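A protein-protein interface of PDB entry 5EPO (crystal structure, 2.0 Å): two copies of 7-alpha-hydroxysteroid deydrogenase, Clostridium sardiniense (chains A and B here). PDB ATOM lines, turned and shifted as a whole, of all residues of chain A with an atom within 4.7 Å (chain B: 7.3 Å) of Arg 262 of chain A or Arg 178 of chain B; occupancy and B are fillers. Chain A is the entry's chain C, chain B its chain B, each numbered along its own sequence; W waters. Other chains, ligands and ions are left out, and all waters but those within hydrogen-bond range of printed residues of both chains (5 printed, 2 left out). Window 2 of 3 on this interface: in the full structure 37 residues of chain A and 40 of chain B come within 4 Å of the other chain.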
ATOM      1  N   ASP A 206      -5.867  16.300 -41.346  1.00  0.00           N
ATOM      2  CA  ASP A 206      -5.270  17.475 -40.707  1.00  0.00           C
ATOM      3  C   ASP A 206      -6.305  18.147 -39.796  1.00  0.00           C
ATOM      4  O   ASP A 206      -6.001  18.549 -38.673  1.00  0.00           O
ATOM      5  CB  ASP A 206      -4.744  18.447 -41.749  1.00  0.00           C
ATOM      6  CG  ASP A 206      -3.480  17.930 -42.416  1.00  0.00           C
ATOM      7  OD1 ASP A 206      -3.220  16.701 -42.339  1.00  0.00           O
ATOM      8  OD2 ASP A 206      -2.724  18.724 -43.023  1.00  0.00           O
ATOM      9  N   LEU A 209      -6.767  15.847 -36.715  1.00  0.00           N
ATOM     10  CA  LEU A 209      -5.632  15.981 -35.809  1.00  0.00           C
ATOM     11  C   LEU A 209      -5.702  17.237 -34.945  1.00  0.00           C
ATOM     12  O   LEU A 209      -5.248  17.231 -33.810  1.00  0.00           O
ATOM     13  CB  LEU A 209      -4.314  15.973 -36.601  1.00  0.00           C
ATOM     14  CG  LEU A 209      -3.027  16.078 -35.799  1.00  0.00           C
ATOM     15  CD1 LEU A 209      -2.924  14.998 -34.758  1.00  0.00           C
ATOM     16  CD2 LEU A 209      -1.807  15.994 -36.716  1.00  0.00           C
ATOM     17  N   GLY A 210      -6.269  18.315 -35.490  1.00  0.00           N
ATOM     18  CA  GLY A 210      -6.381  19.565 -34.748  1.00  0.00           C
ATOM     19  C   GLY A 210      -7.258  19.420 -33.508  1.00  0.00           C
ATOM     20  O   GLY A 210      -7.139  20.214 -32.583  1.00  0.00           O
ATOM     21  N   VAL A 212      -7.340  16.536 -31.709  1.00  0.00           N
ATOM     22  CA  VAL A 212      -6.736  15.510 -30.868  1.00  0.00           C
ATOM     23  C   VAL A 212      -5.885  16.180 -29.780  1.00  0.00           C
ATOM     24  O   VAL A 212      -4.809  16.736 -30.054  1.00  0.00           O
ATOM     25  CB  VAL A 212      -5.857  14.535 -31.695  1.00  0.00           C
ATOM     26  CG1 VAL A 212      -5.224  13.469 -30.825  1.00  0.00           C
ATOM     27  CG2 VAL A 212      -6.688  13.866 -32.785  1.00  0.00           C
ATOM     28  N   PRO A 213      -6.367  16.153 -28.528  1.00  0.00           N
ATOM     29  CA  PRO A 213      -5.638  16.825 -27.460  1.00  0.00           C
ATOM     30  C   PRO A 213      -4.163  16.460 -27.345  1.00  0.00           C
ATOM     31  O   PRO A 213      -3.326  17.354 -27.145  1.00  0.00           O
ATOM     32  CB  PRO A 213      -6.407  16.416 -26.213  1.00  0.00           C
ATOM     33  CG  PRO A 213      -7.805  16.212 -26.689  1.00  0.00           C
ATOM     34  CD  PRO A 213      -7.652  15.595 -28.036  1.00  0.00           C
ATOM     35  N   LEU A 214      -3.839  15.185 -27.462  1.00  0.00           N
ATOM     36  CA  LEU A 214      -2.455  14.756 -27.268  1.00  0.00           C
ATOM     37  C   LEU A 214      -1.625  15.050 -28.506  1.00  0.00           C
ATOM     38  O   LEU A 214      -0.455  14.757 -28.539  1.00  0.00           O
ATOM     39  CB  LEU A 214      -2.395  13.276 -26.874  1.00  0.00           C
ATOM     40  CG  LEU A 214      -2.783  13.028 -25.433  1.00  0.00           C
ATOM     41  CD1 LEU A 214      -3.021  11.540 -25.223  1.00  0.00           C
ATOM     42  CD2 LEU A 214      -1.702  13.560 -24.491  1.00  0.00           C
ATOM     43  N   ASN A 215      -2.264  15.587 -29.532  1.00  0.00           N
ATOM     44  CA  ASN A 215      -1.566  16.311 -30.587  1.00  0.00           C
ATOM     45  C   ASN A 215      -0.618  15.497 -31.437  1.00  0.00           C
ATOM     46  O   ASN A 215       0.451  15.960 -31.808  1.00  0.00           O
ATOM     47  CB  ASN A 215      -0.764  17.496 -29.963  1.00  0.00           C
ATOM     48  CG  ASN A 215      -0.550  18.626 -30.951  1.00  0.00           C
ATOM     49  OD1 ASN A 215      -1.150  18.668 -32.027  1.00  0.00           O
ATOM     50  ND2 ASN A 215       0.316  19.562 -30.593  1.00  0.00           N
ATOM     51  N   TYR A 256     -12.304  23.152 -28.008  1.00  0.00           N
ATOM     52  CA  TYR A 256     -10.934  22.807 -27.671  1.00  0.00           C
ATOM     53  C   TYR A 256      -9.893  23.338 -28.684  1.00  0.00           C
ATOM     54  O   TYR A 256      -8.987  24.089 -28.303  1.00  0.00           O
ATOM     55  CB  TYR A 256     -10.767  21.301 -27.498  1.00  0.00           C
ATOM     56  CG  TYR A 256      -9.357  20.929 -27.106  1.00  0.00           C
ATOM     57  CD1 TYR A 256      -8.926  21.073 -25.796  1.00  0.00           C
ATOM     58  CD2 TYR A 256      -8.422  20.520 -28.056  1.00  0.00           C
ATOM     59  CE1 TYR A 256      -7.636  20.779 -25.422  1.00  0.00           C
ATOM     60  CE2 TYR A 256      -7.145  20.210 -27.702  1.00  0.00           C
ATOM     61  CZ  TYR A 256      -6.736  20.321 -26.414  1.00  0.00           C
ATOM     62  OH  TYR A 256      -5.435  20.016 -26.089  1.00  0.00           O
ATOM     63  N   CYS A 260      -6.974  25.972 -27.845  1.00  0.00           N
ATOM     64  CA  CYS A 260      -5.699  25.290 -27.600  1.00  0.00           C
ATOM     65  C   CYS A 260      -5.069  24.934 -28.932  1.00  0.00           C
ATOM     66  O   CYS A 260      -4.917  23.767 -29.267  1.00  0.00           O
ATOM     67  CB  CYS A 260      -5.922  24.027 -26.752  1.00  0.00           C
ATOM     68  SG  CYS A 260      -6.665  24.341 -25.105  1.00  0.00           S
ATOM     69  N   PRO A 261      -4.708  25.957 -29.713  1.00  0.00           N
ATOM     70  CA  PRO A 261      -4.410  25.707 -31.123  1.00  0.00           C
ATOM     71  C   PRO A 261      -3.043  25.065 -31.280  1.00  0.00           C
ATOM     72  O   PRO A 261      -2.074  25.536 -30.693  1.00  0.00           O
ATOM     73  CB  PRO A 261      -4.478  27.095 -31.754  1.00  0.00           C
ATOM     74  CG  PRO A 261      -4.090  28.023 -30.644  1.00  0.00           C
ATOM     75  CD  PRO A 261      -4.453  27.357 -29.333  1.00  0.00           C
ATOM     76  N   ARG A 262      -3.065  23.954 -31.997  1.00  0.00           N
ATOM     77  CA  ARG A 262      -1.954  23.069 -32.219  1.00  0.00           C
ATOM     78  C   ARG A 262      -0.787  23.806 -32.829  1.00  0.00           C
ATOM     79  O   ARG A 262      -0.944  24.609 -33.759  1.00  0.00           O
ATOM     80  CB  ARG A 262      -2.440  21.919 -33.103  1.00  0.00           C
ATOM     81  CG  ARG A 262      -1.547  21.480 -34.242  1.00  0.00           C
ATOM     82  CD  ARG A 262      -2.275  20.655 -35.243  1.00  0.00           C
ATOM     83  NE  ARG A 262      -3.396  21.376 -35.778  1.00  0.00           N
ATOM     84  CZ  ARG A 262      -4.125  20.964 -36.803  1.00  0.00           C
ATOM     85  NH1 ARG A 262      -5.151  21.711 -37.181  1.00  0.00           N
ATOM     86  NH2 ARG A 262      -3.854  19.833 -37.446  1.00  0.00           N
ATOM     87  OXT ARG A 262       0.311  23.590 -32.350  1.00  0.00           O
ATOM     88  N   GLY B 136       8.577  17.086 -20.219  1.00  0.00           N
ATOM     89  CA  GLY B 136       7.958  16.823 -21.511  1.00  0.00           C
ATOM     90  C   GLY B 136       6.738  15.906 -21.448  1.00  0.00           C
ATOM     91  O   GLY B 136       6.344  15.327 -22.463  1.00  0.00           O
ATOM     92  N   ALA B 173      -7.266  15.930 -17.780  1.00  0.00           N
ATOM     93  CA  ALA B 173      -6.792  15.311 -18.985  1.00  0.00           C
ATOM     94  C   ALA B 173      -6.906  16.251 -20.186  1.00  0.00           C
ATOM     95  O   ALA B 173      -5.973  16.370 -20.990  1.00  0.00           O
ATOM     96  CB  ALA B 173      -7.570  14.014 -19.281  1.00  0.00           C
ATOM     97  N   LEU B 174      -8.051  16.922 -20.302  1.00  0.00           N
ATOM     98  CA  LEU B 174      -8.264  17.807 -21.425  1.00  0.00           C
ATOM     99  C   LEU B 174      -7.333  19.046 -21.338  1.00  0.00           C
ATOM    100  O   LEU B 174      -6.810  19.527 -22.337  1.00  0.00           O
ATOM    101  CB  LEU B 174      -9.693  18.247 -21.500  1.00  0.00           C
ATOM    102  CG  LEU B 174     -10.091  19.074 -22.725  1.00  0.00           C
ATOM    103  CD1 LEU B 174      -9.986  18.215 -23.972  1.00  0.00           C
ATOM    104  CD2 LEU B 174     -11.478  19.663 -22.532  1.00  0.00           C
ATOM    105  N   GLN B 175      -7.138  19.513 -20.112  1.00  0.00           N
ATOM    106  CA  GLN B 175      -6.454  20.795 -19.864  1.00  0.00           C
ATOM    107  C   GLN B 175      -4.927  20.699 -20.062  1.00  0.00           C
ATOM    108  O   GLN B 175      -4.309  21.705 -20.339  1.00  0.00           O
ATOM    109  CB  GLN B 175      -6.782  21.295 -18.477  1.00  0.00           C
ATOM    110  CG  GLN B 175      -8.152  21.920 -18.366  1.00  0.00           C
ATOM    111  CD  GLN B 175      -8.665  22.095 -16.955  1.00  0.00           C
ATOM    112  OE1 GLN B 175      -7.916  22.102 -15.989  1.00  0.00           O
ATOM    113  NE2 GLN B 175      -9.987  22.175 -16.825  1.00  0.00           N
ATOM    114  N   TYR B 176      -4.334  19.524 -19.922  1.00  0.00           N
ATOM    115  CA  TYR B 176      -2.877  19.399 -19.993  1.00  0.00           C
ATOM    116  C   TYR B 176      -2.374  18.420 -21.041  1.00  0.00           C
ATOM    117  O   TYR B 176      -1.186  18.139 -21.123  1.00  0.00           O
ATOM    118  CB  TYR B 176      -2.311  19.101 -18.592  1.00  0.00           C
ATOM    119  CG  TYR B 176      -2.688  20.238 -17.655  1.00  0.00           C
ATOM    120  CD1 TYR B 176      -1.940  21.412 -17.613  1.00  0.00           C
ATOM    121  CD2 TYR B 176      -3.877  20.189 -16.917  1.00  0.00           C
ATOM    122  CE1 TYR B 176      -2.332  22.485 -16.826  1.00  0.00           C
ATOM    123  CE2 TYR B 176      -4.268  21.249 -16.116  1.00  0.00           C
ATOM    124  CZ  TYR B 176      -3.479  22.411 -16.075  1.00  0.00           C
ATOM    125  OH  TYR B 176      -3.869  23.472 -15.313  1.00  0.00           O
ATOM    126  N   ALA B 177      -3.291  17.962 -21.901  1.00  0.00           N
ATOM    127  CA  ALA B 177      -2.921  17.145 -23.045  1.00  0.00           C
ATOM    128  C   ALA B 177      -1.891  17.812 -23.930  1.00  0.00           C
ATOM    129  O   ALA B 177      -1.012  17.113 -24.486  1.00  0.00           O
ATOM    130  CB  ALA B 177      -4.133  16.764 -23.859  1.00  0.00           C
ATOM    131  N   ARG B 178      -1.953  19.154 -24.071  1.00  0.00           N
ATOM    132  CA  ARG B 178      -0.966  19.801 -24.972  1.00  0.00           C
ATOM    133  C   ARG B 178       0.437  19.685 -24.419  1.00  0.00           C
ATOM    134  O   ARG B 178       1.404  19.840 -25.143  1.00  0.00           O
ATOM    135  CB  ARG B 178      -1.293  21.267 -25.218  1.00  0.00           C
ATOM    136  CG  ARG B 178      -2.497  21.548 -26.082  1.00  0.00           C
ATOM    137  CD  ARG B 178      -2.534  20.735 -27.340  1.00  0.00           C
ATOM    138  NE  ARG B 178      -3.372  21.326 -28.385  1.00  0.00           N
ATOM    139  CZ  ARG B 178      -3.946  20.619 -29.357  1.00  0.00           C
ATOM    140  NH1 ARG B 178      -3.802  19.292 -29.405  1.00  0.00           N
ATOM    141  NH2 ARG B 178      -4.676  21.232 -30.287  1.00  0.00           N
ATOM    142  N   LYS B 179       0.543  19.430 -23.122  1.00  0.00           N
ATOM    143  CA  LYS B 179       1.838  19.284 -22.473  1.00  0.00           C
ATOM    144  C   LYS B 179       2.249  17.824 -22.326  1.00  0.00           C
ATOM    145  O   LYS B 179       3.230  17.513 -21.633  1.00  0.00           O
ATOM    146  CB  LYS B 179       1.807  19.983 -21.108  1.00  0.00           C
ATOM    147  CG  LYS B 179       1.607  21.486 -21.171  1.00  0.00           C
ATOM    148  CD  LYS B 179       2.728  22.146 -21.958  1.00  0.00           C
ATOM    149  CE  LYS B 179       2.873  23.640 -21.714  1.00  0.00           C
ATOM    150  NZ  LYS B 179       1.902  24.435 -22.496  1.00  0.00           N
ATOM    151  N   ASN B 180       1.481  16.924 -22.958  1.00  0.00           N
ATOM    152  CA  ASN B 180       1.709  15.498 -22.892  1.00  0.00           C
ATOM    153  C   ASN B 180       1.573  14.951 -21.463  1.00  0.00           C
ATOM    154  O   ASN B 180       2.170  13.938 -21.102  1.00  0.00           O
ATOM    155  CB  ASN B 180       3.080  15.142 -23.466  1.00  0.00           C
ATOM    156  CG  ASN B 180       3.191  13.660 -23.819  1.00  0.00           C
ATOM    157  OD1 ASN B 180       2.255  13.060 -24.361  1.00  0.00           O
ATOM    158  ND2 ASN B 180       4.316  13.037 -23.450  1.00  0.00           N
ATOM    159  N   ILE B 181       0.752  15.630 -20.665  1.00  0.00           N
ATOM    160  CA  ILE B 181       0.390  15.146 -19.358  1.00  0.00           C
ATOM    161  C   ILE B 181      -0.979  14.449 -19.480  1.00  0.00           C
ATOM    162  O   ILE B 181      -1.952  15.067 -19.895  1.00  0.00           O
ATOM    163  CB  ILE B 181       0.306  16.293 -18.350  1.00  0.00           C
ATOM    164  CG1 ILE B 181       1.679  16.955 -18.246  1.00  0.00           C
ATOM    165  CG2 ILE B 181      -0.183  15.776 -16.969  1.00  0.00           C
ATOM    166  CD1 ILE B 181       1.732  18.192 -17.366  1.00  0.00           C
HETATM  167  O   HOH W   1       1.350  12.963 -26.989  1.00  0.00           O
HETATM  168  O   HOH W   2       0.635  16.743 -26.651  1.00  0.00           O
HETATM  169  O   HOH W   3      -5.776  22.937 -32.602  1.00  0.00           O
HETATM  170  O   HOH W   4      -4.588  20.622 -23.614  1.00  0.00           O
HETATM  171  O   HOH W   5      -3.684  22.991 -23.455  1.00  0.00           O
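The backbone carbonyl oxygen (O) of Gly 136 of chain B lies within hydrogen-bond range of the side-chain amide nitrogen (ND2) of Asn 180 of chain B (3.2 Å).
The guanidinium group of Arg 262 of chain A sits at hydrogen-bond distance from the backbone carbonyl oxygen of Asp 206 of chain A (2.8 Å).
Asp 206 of chain A touches none of the printed residues of chain B.
Printed residues of chain B within 4 Å of Asn 215 of chain A: Arg 178.
Of chain B, only Arg 178 (3.6 Å) comes within 4 Å of Arg 262 of chain A.
Printed residues of chain A within 4 Å of Ala 177 of chain B: Pro 213 (3.3 Å) and Leu 214 (3.6 Å).
Of the printed residues of chain A, Arg 178 of chain B touches Gly 210 (3.5 Å), Val 212 (2.8 Å), Pro 213 (3.0 Å), Asn 215 (3.6 Å), Tyr 256 (3.2 Å), Cys 260 (2.7 Å) and Arg 262 (3.6 Å).
The nearest printed residue of chain B that does not touch Arg 262 of chain A is Ala 177 of chain B (9.8 Å).
The nearest residue of chain A that does not touch Arg 178 of chain B is Pro 261 of chain A (4.3 Å).
Water W4 lies within hydrogen-bond range of OH of Tyr 256 of chain A (2.7 Å), O of Leu 174 of chain B (2.8 Å), N of Arg 178 of chain B (3.1 Å), N of Ala 177 of chain B (3.4 Å) and O of Gln 175 of chain B (3.5 Å).
Water W2 lies within hydrogen-bond range of O of Ala 177 of chain B (2.7 Å) and O of Leu 214 of chain A (2.9 Å).
Water W1 lies within hydrogen-bond range of the side-chain amide oxygen of Asn 180 of chain B and the backbone carbonyl oxygen of Leu 214 of chain A.
Water W3 lies within hydrogen-bond range of N of Arg 262 of chain A (3.0 Å), O of Gly 210 of chain A (3.0 Å) and NH2 of Arg 178 of chain B (3.1 Å).
Water W5 bridges the backbone carbonyl oxygen (O) of Gln 175 of chain B (3.4 Å) and the side-chain sulfur (SG) of Cys 260 of chain A (3.7 Å).
NH1 of Arg 178 of chain B lies within hydrogen-bond range of O of Val 212 of chain A (2.8 Å).
O of Pro 213 of chain A lies within hydrogen-bond range of NH1 of Arg 178 of chain B (3.0 Å).
The guanidinium group of Arg 178 of chain B sits close to the side-chain hydroxyl of Tyr 256 of chain A, at 3.4 Å.
The backbone carbonyl oxygen (O) of Cys 260 of chain A sits at hydrogen-bond distance from the guanidinium group (NH2) of Arg 178 of chain B (2.7 Å).
Printed residues of chain A that touch a printed residue of chain B: Gly 210, Val 212, Pro 213, Leu 214, Asn 215, Tyr 256, Cys 260 and Arg 262.
Of the 10 printed residues of chain B, 4 touch a printed residue of chain A.
Hydrophobic or aromatic side chains of chain B within 4 Å of the printed part of chain A: Leu 174 and Ala 177.
Among the printed residues, 11 pairs touch across the chains.
Among the printed residues, no Asp or Glu carboxylate lies within 4 Å of a Lys or Arg side-chain nitrogen of the other chain.
No position is printed for both chains.
Of the 11 pairs that touch across the chains among the printed residues, none has its exchanged pair printed and touching as well.
Among the printed residues, merely in contact across the chains: Gly 210 of chain A with Arg 178 of chain B (3.5 Å), Pro 213 of chain A with Ala 177 of chain B (3.3 Å), Leu 214 of chain A with Ala 177 of chain B (3.6 Å), Leu 214 of chain A with Asn 180 of chain B (3.99 Å), Asn 215 of chain A with Arg 178 of chain B (3.6 Å), Tyr 256 of chain A with Leu 174 of chain B (3.4 Å) and Arg 262 of chain A with Arg 178 of chain B (3.6 Å).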
